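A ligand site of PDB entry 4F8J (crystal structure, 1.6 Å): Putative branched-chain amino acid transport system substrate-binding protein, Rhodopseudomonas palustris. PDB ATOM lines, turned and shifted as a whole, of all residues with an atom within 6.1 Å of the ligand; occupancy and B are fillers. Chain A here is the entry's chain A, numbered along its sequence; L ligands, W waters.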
ATOM      1  N   LEU A  23      -9.145  -2.706  32.577  1.00  0.00           N
ATOM      2  CA  LEU A  23      -9.076  -1.760  31.448  1.00  0.00           C
ATOM      3  C   LEU A  23      -9.540  -0.365  31.861  1.00  0.00           C
ATOM      4  O   LEU A  23      -8.923   0.644  31.543  1.00  0.00           O
ATOM      5  CB  LEU A  23      -9.949  -2.241  30.241  1.00  0.00           C
ATOM      6  CG  LEU A  23      -9.301  -3.348  29.399  1.00  0.00           C
ATOM      7  CD1 LEU A  23      -9.309  -4.663  30.159  1.00  0.00           C
ATOM      8  CD2 LEU A  23      -9.968  -3.531  28.048  1.00  0.00           C
ATOM      9  N   GLU A  27      -7.839   3.804  32.569  1.00  0.00           N
ATOM     10  CA  GLU A  27      -8.427   4.861  31.741  1.00  0.00           C
ATOM     11  C   GLU A  27      -8.879   6.013  32.621  1.00  0.00           C
ATOM     12  O   GLU A  27      -8.671   7.186  32.292  1.00  0.00           O
ATOM     13  CB  GLU A  27      -9.570   4.291  30.884  1.00  0.00           C
ATOM     14  CG  GLU A  27      -8.972   3.423  29.816  1.00  0.00           C
ATOM     15  CD  GLU A  27      -9.876   2.518  29.043  1.00  0.00           C
ATOM     16  OE1 GLU A  27     -11.078   2.387  29.357  1.00  0.00           O
ATOM     17  OE2 GLU A  27      -9.315   1.871  28.105  1.00  0.00           O
ATOM     18  N   SER A  77     -14.826   0.859  27.856  1.00  0.00           N
ATOM     19  CA  SER A  77     -13.575   0.148  27.993  1.00  0.00           C
ATOM     20  C   SER A  77     -13.512  -1.126  27.151  1.00  0.00           C
ATOM     21  O   SER A  77     -12.418  -1.603  26.801  1.00  0.00           O
ATOM     22  CB  SER A  77     -13.356  -0.211  29.471  1.00  0.00           C
ATOM     23  OG  SER A  77     -13.234   0.953  30.253  1.00  0.00           O
ATOM     24  N   VAL A  78     -14.672  -1.703  26.874  1.00  0.00           N
ATOM     25  CA  VAL A  78     -14.804  -2.933  26.084  1.00  0.00           C
ATOM     26  C   VAL A  78     -15.876  -2.761  25.014  1.00  0.00           C
ATOM     27  O   VAL A  78     -16.603  -1.766  25.045  1.00  0.00           O
ATOM     28  CB  VAL A  78     -15.035  -4.176  26.957  1.00  0.00           C
ATOM     29  CG1 VAL A  78     -13.787  -4.498  27.773  1.00  0.00           C
ATOM     30  CG2 VAL A  78     -16.274  -4.041  27.839  1.00  0.00           C
ATOM     31  N   THR A  79     -15.931  -3.671  24.039  1.00  0.00           N
ATOM     32  CA  THR A  79     -16.671  -3.374  22.818  1.00  0.00           C
ATOM     33  C   THR A  79     -18.190  -3.232  23.049  1.00  0.00           C
ATOM     34  O   THR A  79     -18.788  -2.286  22.562  1.00  0.00           O
ATOM     35  CB  THR A  79     -16.336  -4.361  21.686  1.00  0.00           C
ATOM     36  OG1 THR A  79     -14.956  -4.206  21.380  1.00  0.00           O
ATOM     37  CG2 THR A  79     -17.186  -4.081  20.438  1.00  0.00           C
ATOM     38  N   PRO A  80     -18.827  -4.163  23.764  1.00  0.00           N
ATOM     39  CA  PRO A  80     -20.290  -4.079  23.874  1.00  0.00           C
ATOM     40  C   PRO A  80     -20.836  -2.740  24.403  1.00  0.00           C
ATOM     41  O   PRO A  80     -21.732  -2.190  23.774  1.00  0.00           O
ATOM     42  CB  PRO A  80     -20.664  -5.324  24.711  1.00  0.00           C
ATOM     43  CG  PRO A  80     -19.538  -6.244  24.456  1.00  0.00           C
ATOM     44  CD  PRO A  80     -18.308  -5.429  24.327  1.00  0.00           C
ATOM     45  N   LEU A  99     -13.125   4.230  23.272  1.00  0.00           N
ATOM     46  CA  LEU A  99     -11.931   3.761  23.977  1.00  0.00           C
ATOM     47  C   LEU A  99     -11.765   2.230  23.846  1.00  0.00           C
ATOM     48  O   LEU A  99     -10.838   1.676  24.431  1.00  0.00           O
ATOM     49  CB  LEU A  99     -11.936   4.273  25.433  1.00  0.00           C
ATOM     50  CG  LEU A  99     -12.044   5.769  25.640  1.00  0.00           C
ATOM     51  CD1 LEU A  99     -12.028   6.111  27.159  1.00  0.00           C
ATOM     52  CD2 LEU A  99     -10.938   6.558  24.872  1.00  0.00           C
ATOM     53  N   ALA A 100     -12.642   1.598  23.075  1.00  0.00           N
ATOM     54  CA  ALA A 100     -12.557   0.193  22.663  1.00  0.00           C
ATOM     55  C   ALA A 100     -12.787   0.106  21.168  1.00  0.00           C
ATOM     56  O   ALA A 100     -13.462   0.968  20.594  1.00  0.00           O
ATOM     57  CB  ALA A 100     -13.576  -0.643  23.421  1.00  0.00           C
ATOM     58  N   PRO A 101     -12.240  -0.906  20.457  1.00  0.00           N
ATOM     59  CA  PRO A 101     -12.260  -0.861  18.967  1.00  0.00           C
ATOM     60  C   PRO A 101     -13.531  -1.491  18.310  1.00  0.00           C
ATOM     61  O   PRO A 101     -13.451  -2.566  17.722  1.00  0.00           O
ATOM     62  CB  PRO A 101     -10.969  -1.611  18.576  1.00  0.00           C
ATOM     63  CG  PRO A 101     -10.808  -2.606  19.659  1.00  0.00           C
ATOM     64  CD  PRO A 101     -11.426  -2.037  20.934  1.00  0.00           C
ATOM     65  N   PRO A 116      -8.480   3.103  19.977  1.00  0.00           N
ATOM     66  CA  PRO A 116      -7.717   1.838  19.805  1.00  0.00           C
ATOM     67  C   PRO A 116      -7.389   1.542  18.367  1.00  0.00           C
ATOM     68  O   PRO A 116      -8.144   1.887  17.462  1.00  0.00           O
ATOM     69  CB  PRO A 116      -8.644   0.773  20.381  1.00  0.00           C
ATOM     70  CG  PRO A 116      -9.495   1.540  21.339  1.00  0.00           C
ATOM     71  CD  PRO A 116      -9.775   2.825  20.644  1.00  0.00           C
ATOM     72  N   GLN A 117      -6.274   0.855  18.152  1.00  0.00           N
ATOM     73  CA  GLN A 117      -5.917   0.456  16.827  1.00  0.00           C
ATOM     74  C   GLN A 117      -6.966  -0.455  16.201  1.00  0.00           C
ATOM     75  O   GLN A 117      -7.504  -1.351  16.889  1.00  0.00           O
ATOM     76  CB  GLN A 117      -4.579  -0.241  16.820  1.00  0.00           C
ATOM     77  CG  GLN A 117      -3.386   0.621  17.261  1.00  0.00           C
ATOM     78  CD  GLN A 117      -3.235   0.771  18.747  1.00  0.00           C
ATOM     79  OE1 GLN A 117      -3.975   0.191  19.547  1.00  0.00           O
ATOM     80  NE2 GLN A 117      -2.269   1.603  19.141  1.00  0.00           N
ATOM     81  N   TYR A 143     -13.617 -14.474  22.073  1.00  0.00           N
ATOM     82  CA  TYR A 143     -14.965 -14.260  22.606  1.00  0.00           C
ATOM     83  C   TYR A 143     -16.028 -14.642  21.598  1.00  0.00           C
ATOM     84  O   TYR A 143     -15.859 -14.447  20.386  1.00  0.00           O
ATOM     85  CB  TYR A 143     -15.207 -12.809  22.966  1.00  0.00           C
ATOM     86  CG  TYR A 143     -14.317 -12.232  24.030  1.00  0.00           C
ATOM     87  CD1 TYR A 143     -13.937 -12.966  25.143  1.00  0.00           C
ATOM     88  CD2 TYR A 143     -13.972 -10.899  24.001  1.00  0.00           C
ATOM     89  CE1 TYR A 143     -13.142 -12.410  26.151  1.00  0.00           C
ATOM     90  CE2 TYR A 143     -13.172 -10.321  24.968  1.00  0.00           C
ATOM     91  CZ  TYR A 143     -12.787 -11.062  26.060  1.00  0.00           C
ATOM     92  OH  TYR A 143     -11.999 -10.504  27.061  1.00  0.00           O
ATOM     93  N   ASP A 145     -18.564 -12.910  20.850  1.00  0.00           N
ATOM     94  CA  ASP A 145     -19.278 -11.664  20.655  1.00  0.00           C
ATOM     95  C   ASP A 145     -18.561 -10.863  19.559  1.00  0.00           C
ATOM     96  O   ASP A 145     -17.649 -11.384  18.909  1.00  0.00           O
ATOM     97  CB  ASP A 145     -19.381 -10.888  21.991  1.00  0.00           C
ATOM     98  CG  ASP A 145     -18.072 -10.266  22.446  1.00  0.00           C
ATOM     99  OD1 ASP A 145     -17.035 -10.309  21.757  1.00  0.00           O
ATOM    100  OD2 ASP A 145     -18.104  -9.715  23.564  1.00  0.00           O
ATOM    101  N   TYR A 147     -16.292  -8.404  19.322  1.00  0.00           N
ATOM    102  CA  TYR A 147     -14.827  -8.329  19.359  1.00  0.00           C
ATOM    103  C   TYR A 147     -14.196  -9.650  18.895  1.00  0.00           C
ATOM    104  O   TYR A 147     -13.254  -9.660  18.081  1.00  0.00           O
ATOM    105  CB  TYR A 147     -14.327  -7.925  20.739  1.00  0.00           C
ATOM    106  CG  TYR A 147     -12.829  -7.775  20.876  1.00  0.00           C
ATOM    107  CD1 TYR A 147     -12.194  -6.671  20.358  1.00  0.00           C
ATOM    108  CD2 TYR A 147     -12.041  -8.722  21.534  1.00  0.00           C
ATOM    109  CE1 TYR A 147     -10.826  -6.514  20.478  1.00  0.00           C
ATOM    110  CE2 TYR A 147     -10.666  -8.583  21.643  1.00  0.00           C
ATOM    111  CZ  TYR A 147     -10.066  -7.455  21.107  1.00  0.00           C
ATOM    112  OH  TYR A 147      -8.725  -7.245  21.196  1.00  0.00           O
ATOM    113  N   ARG A 174     -17.020 -13.944  27.917  1.00  0.00           N
ATOM    114  CA  ARG A 174     -16.216 -13.100  28.794  1.00  0.00           C
ATOM    115  C   ARG A 174     -16.183 -13.576  30.248  1.00  0.00           C
ATOM    116  O   ARG A 174     -15.116 -13.634  30.854  1.00  0.00           O
ATOM    117  CB  ARG A 174     -16.703 -11.642  28.732  1.00  0.00           C
ATOM    118  CG  ARG A 174     -16.332 -10.948  27.444  1.00  0.00           C
ATOM    119  CD  ARG A 174     -17.083  -9.631  27.272  1.00  0.00           C
ATOM    120  NE  ARG A 174     -16.863  -9.113  25.927  1.00  0.00           N
ATOM    121  CZ  ARG A 174     -15.882  -8.265  25.580  1.00  0.00           C
ATOM    122  NH1 ARG A 174     -15.753  -7.934  24.313  1.00  0.00           N
ATOM    123  NH2 ARG A 174     -15.042  -7.799  26.496  1.00  0.00           N
ATOM    124  N   ALA A 198      -9.202 -11.911  22.830  1.00  0.00           N
ATOM    125  CA  ALA A 198      -9.821 -11.596  24.099  1.00  0.00           C
ATOM    126  C   ALA A 198      -9.092 -10.356  24.631  1.00  0.00           C
ATOM    127  O   ALA A 198      -8.372  -9.686  23.872  1.00  0.00           O
ATOM    128  CB  ALA A 198      -9.719 -12.799  25.047  1.00  0.00           C
ATOM    129  N   SER A 199      -9.326 -10.032  25.907  1.00  0.00           N
ATOM    130  CA  SER A 199      -8.824  -8.785  26.458  1.00  0.00           C
ATOM    131  C   SER A 199      -8.706  -8.901  27.964  1.00  0.00           C
ATOM    132  O   SER A 199      -9.346  -9.741  28.566  1.00  0.00           O
ATOM    133  CB  SER A 199      -9.762  -7.639  26.071  1.00  0.00           C
ATOM    134  OG  SER A 199     -11.060  -7.842  26.607  1.00  0.00           O
ATOM    135  N   THR A 222      -3.872 -10.395  21.215  1.00  0.00           N
ATOM    136  CA  THR A 222      -4.336  -9.110  20.703  1.00  0.00           C
ATOM    137  C   THR A 222      -3.947  -7.940  21.615  1.00  0.00           C
ATOM    138  O   THR A 222      -3.459  -8.115  22.752  1.00  0.00           O
ATOM    139  CB  THR A 222      -5.888  -9.058  20.528  1.00  0.00           C
ATOM    140  OG1 THR A 222      -6.555  -8.915  21.784  1.00  0.00           O
ATOM    141  CG2 THR A 222      -6.442 -10.252  19.789  1.00  0.00           C
ATOM    142  N   HIS A 223      -4.162  -6.727  21.104  1.00  0.00           N
ATOM    143  CA  HIS A 223      -3.872  -5.516  21.868  1.00  0.00           C
ATOM    144  C   HIS A 223      -4.800  -5.301  23.051  1.00  0.00           C
ATOM    145  O   HIS A 223      -4.496  -4.547  23.965  1.00  0.00           O
ATOM    146  CB  HIS A 223      -3.767  -4.304  20.980  1.00  0.00           C
ATOM    147  CG  HIS A 223      -4.964  -4.045  20.101  1.00  0.00           C
ATOM    148  ND1 HIS A 223      -5.678  -5.030  19.465  1.00  0.00           N
ATOM    149  CD2 HIS A 223      -5.489  -2.841  19.652  1.00  0.00           C
ATOM    150  CE1 HIS A 223      -6.629  -4.447  18.702  1.00  0.00           C
ATOM    151  NE2 HIS A 223      -6.523  -3.116  18.823  1.00  0.00           N
ATOM    152  N   GLY A 224      -5.873  -6.033  23.097  1.00  0.00           N
ATOM    153  CA  GLY A 224      -6.706  -6.083  24.293  1.00  0.00           C
ATOM    154  C   GLY A 224      -6.018  -6.636  25.540  1.00  0.00           C
ATOM    155  O   GLY A 224      -6.560  -6.512  26.649  1.00  0.00           O
ATOM    156  N   ALA A 225      -4.852  -7.280  25.372  1.00  0.00           N
ATOM    157  CA  ALA A 225      -4.091  -7.907  26.464  1.00  0.00           C
ATOM    158  C   ALA A 225      -2.923  -7.072  26.977  1.00  0.00           C
ATOM    159  O   ALA A 225      -2.243  -7.500  27.903  1.00  0.00           O
ATOM    160  CB  ALA A 225      -3.552  -9.283  26.001  1.00  0.00           C
ATOM    161  N   GLN A 282      -1.753  -0.229  27.660  1.00  0.00           N
ATOM    162  CA  GLN A 282      -2.521   0.059  26.435  1.00  0.00           C
ATOM    163  C   GLN A 282      -3.715   0.989  26.727  1.00  0.00           C
ATOM    164  O   GLN A 282      -4.007   1.884  25.960  1.00  0.00           O
ATOM    165  CB  GLN A 282      -3.014  -1.267  25.857  1.00  0.00           C
ATOM    166  CG  GLN A 282      -3.861  -1.187  24.598  1.00  0.00           C
ATOM    167  CD  GLN A 282      -3.095  -0.946  23.331  1.00  0.00           C
ATOM    168  OE1 GLN A 282      -1.875  -0.763  23.331  1.00  0.00           O
ATOM    169  NE2 GLN A 282      -3.839  -0.900  22.205  1.00  0.00           N
ATOM    170  N   PHE A 283      -4.358   0.759  27.870  1.00  0.00           N
ATOM    171  CA  PHE A 283      -5.684   1.321  28.164  1.00  0.00           C
ATOM    172  C   PHE A 283      -5.616   2.771  28.667  1.00  0.00           C
ATOM    173  O   PHE A 283      -6.334   3.652  28.178  1.00  0.00           O
ATOM    174  CB  PHE A 283      -6.409   0.381  29.138  1.00  0.00           C
ATOM    175  CG  PHE A 283      -6.244  -1.083  28.749  1.00  0.00           C
ATOM    176  CD1 PHE A 283      -6.650  -1.510  27.484  1.00  0.00           C
ATOM    177  CD2 PHE A 283      -5.587  -1.956  29.586  1.00  0.00           C
ATOM    178  CE1 PHE A 283      -6.467  -2.845  27.096  1.00  0.00           C
ATOM    179  CE2 PHE A 283      -5.395  -3.277  29.180  1.00  0.00           C
ATOM    180  CZ  PHE A 283      -5.836  -3.692  27.937  1.00  0.00           C
ATOM    181  N   HIS A 286      -5.405   5.269  25.914  1.00  0.00           N
ATOM    182  CA  HIS A 286      -6.552   5.664  25.092  1.00  0.00           C
ATOM    183  C   HIS A 286      -7.265   6.893  25.623  1.00  0.00           C
ATOM    184  O   HIS A 286      -7.622   7.785  24.846  1.00  0.00           O
ATOM    185  CB  HIS A 286      -7.539   4.557  24.856  1.00  0.00           C
ATOM    186  CG  HIS A 286      -6.952   3.346  24.169  1.00  0.00           C
ATOM    187  ND1 HIS A 286      -6.032   3.430  23.164  1.00  0.00           N
ATOM    188  CD2 HIS A 286      -7.176   1.973  24.395  1.00  0.00           C
ATOM    189  CE1 HIS A 286      -5.699   2.185  22.757  1.00  0.00           C
ATOM    190  NE2 HIS A 286      -6.400   1.299  23.473  1.00  0.00           N
ATOM    191  N   GLN A 330      -0.322   6.555  21.253  1.00  0.00           N
ATOM    192  CA  GLN A 330      -0.597   5.290  20.585  1.00  0.00           C
ATOM    193  C   GLN A 330      -0.511   5.322  19.078  1.00  0.00           C
ATOM    194  O   GLN A 330      -0.676   4.291  18.423  1.00  0.00           O
ATOM    195  CB  GLN A 330      -1.970   4.756  21.012  1.00  0.00           C
ATOM    196  CG  GLN A 330      -2.050   4.354  22.478  1.00  0.00           C
ATOM    197  CD  GLN A 330      -1.395   3.032  22.764  1.00  0.00           C
ATOM    198  OE1 GLN A 330      -0.234   2.826  22.391  1.00  0.00           O
ATOM    199  NE2 GLN A 330      -2.126   2.110  23.402  1.00  0.00           N
HETATM  200  C1  LIG L   1     -13.004  -5.837  24.139  1.00  0.00           C
HETATM  201  O1  LIG L   1     -14.113  -5.779  23.586  1.00  0.00           O
HETATM  202  O2  LIG L   1     -12.843  -6.425  25.241  1.00  0.00           O
HETATM  203  C2  LIG L   1     -11.776  -5.228  23.561  1.00  0.00           C
HETATM  204  C3  LIG L   1     -11.025  -4.468  24.356  1.00  0.00           C
HETATM  205  C4  LIG L   1      -9.871  -3.650  23.869  1.00  0.00           C
HETATM  206  C5  LIG L   1      -9.036  -4.023  22.789  1.00  0.00           C
HETATM  207  C6  LIG L   1      -8.034  -3.172  22.353  1.00  0.00           C
HETATM  208  C7  LIG L   1      -7.781  -1.956  22.959  1.00  0.00           C
HETATM  209  C8  LIG L   1      -8.579  -1.592  24.032  1.00  0.00           C
HETATM  210  C9  LIG L   1      -9.589  -2.444  24.447  1.00  0.00           C
HETATM  211  O3  LIG L   1      -6.768  -1.112  22.568  1.00  0.00           O
HETATM  212  O   HOH W   1     -10.367   0.158  26.537  1.00  0.00           O
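A ring nitrogen (NE2) of His 286 lies within hydrogen-bond range of an oxygen (O3) of the ligand.
An oxygen (O2) of the ligand lies within hydrogen-bond range of the side-chain hydroxyl of Ser 199.
O1 of the ligand is in salt-bridge range of NH1 of Arg 174 (2.8 Å).
N of Thr 79 is in hydrogen-bond range of O1 of the ligand (2.8 Å).
OG1 of Thr 79 is in hydrogen-bond range of O1 of the ligand, at 2.8 Å.
The side-chain amide nitrogen (NE2) of Gln 282 lies within hydrogen-bond range of an oxygen (O3) of the ligand, 3.0 Å away.
The side-chain hydroxyl (OH) of Tyr 143 is in hydrogen-bond range of the side-chain hydroxyl (OG) of Ser 199 (2.9 Å).
The guanidinium group (NE) of Arg 174 is in salt-bridge range of the side-chain carboxylate (OD2) of Asp 145 (2.7 Å).
The side-chain amide oxygen (OE1) of Gln 282 lies within hydrogen-bond range of the side-chain amide nitrogen (NE2) of Gln 330 (2.9 Å).
The backbone NH (N) of Gly 224 sits close to the side-chain hydroxyl (OG1) of Thr 222, at 3.2 Å.
OG1 of Thr 222 sits at hydrogen-bond distance from OH of Tyr 147, at 2.8 Å.
The backbone NH (N) of Tyr 147 is in hydrogen-bond range of the side-chain carboxylate (OD1) of Asp 145 (3.2 Å).
A ring nitrogen (NE2) of His 223 sits at hydrogen-bond distance from the backbone carbonyl oxygen (O) of Gln 117 (2.8 Å).
OE1 of Glu 27 is in hydrogen-bond range of OG of Ser 77 (2.7 Å).
Leu 23 touches the ligand (CD2 to C9, 3.8 Å).
O of Ser 77 touches C9 of the ligand, at 3.8 Å.
CG1 of Val 78 touches O2 of the ligand, 3.3 Å away.
O of Leu 99 touches C8 of the ligand (3.99 Å).
Pro 101 touches the ligand (CD to C5, 3.6 Å).
Pro 116 touches the ligand.
Tyr 143 touches the ligand (CE2 to O2, 3.9 Å).
CE1 of Tyr 147 touches C2 of the ligand, at 3.5 Å.
His 223 touches the ligand.
CA of Gly 224 touches C5 of the ligand, at 3.5 Å.
CE1 of Phe 283 touches C8 of the ligand (3.9 Å).
Hydrophobic or aromatic side chains within 4 Å of the ligand: Leu 23, Val 78, Pro 101, Pro 116, Tyr 143, Tyr 147, His 223, Phe 283 and His 286.
The nearest printed residue that does not touch the ligand is Pro 80 (4.3 Å).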
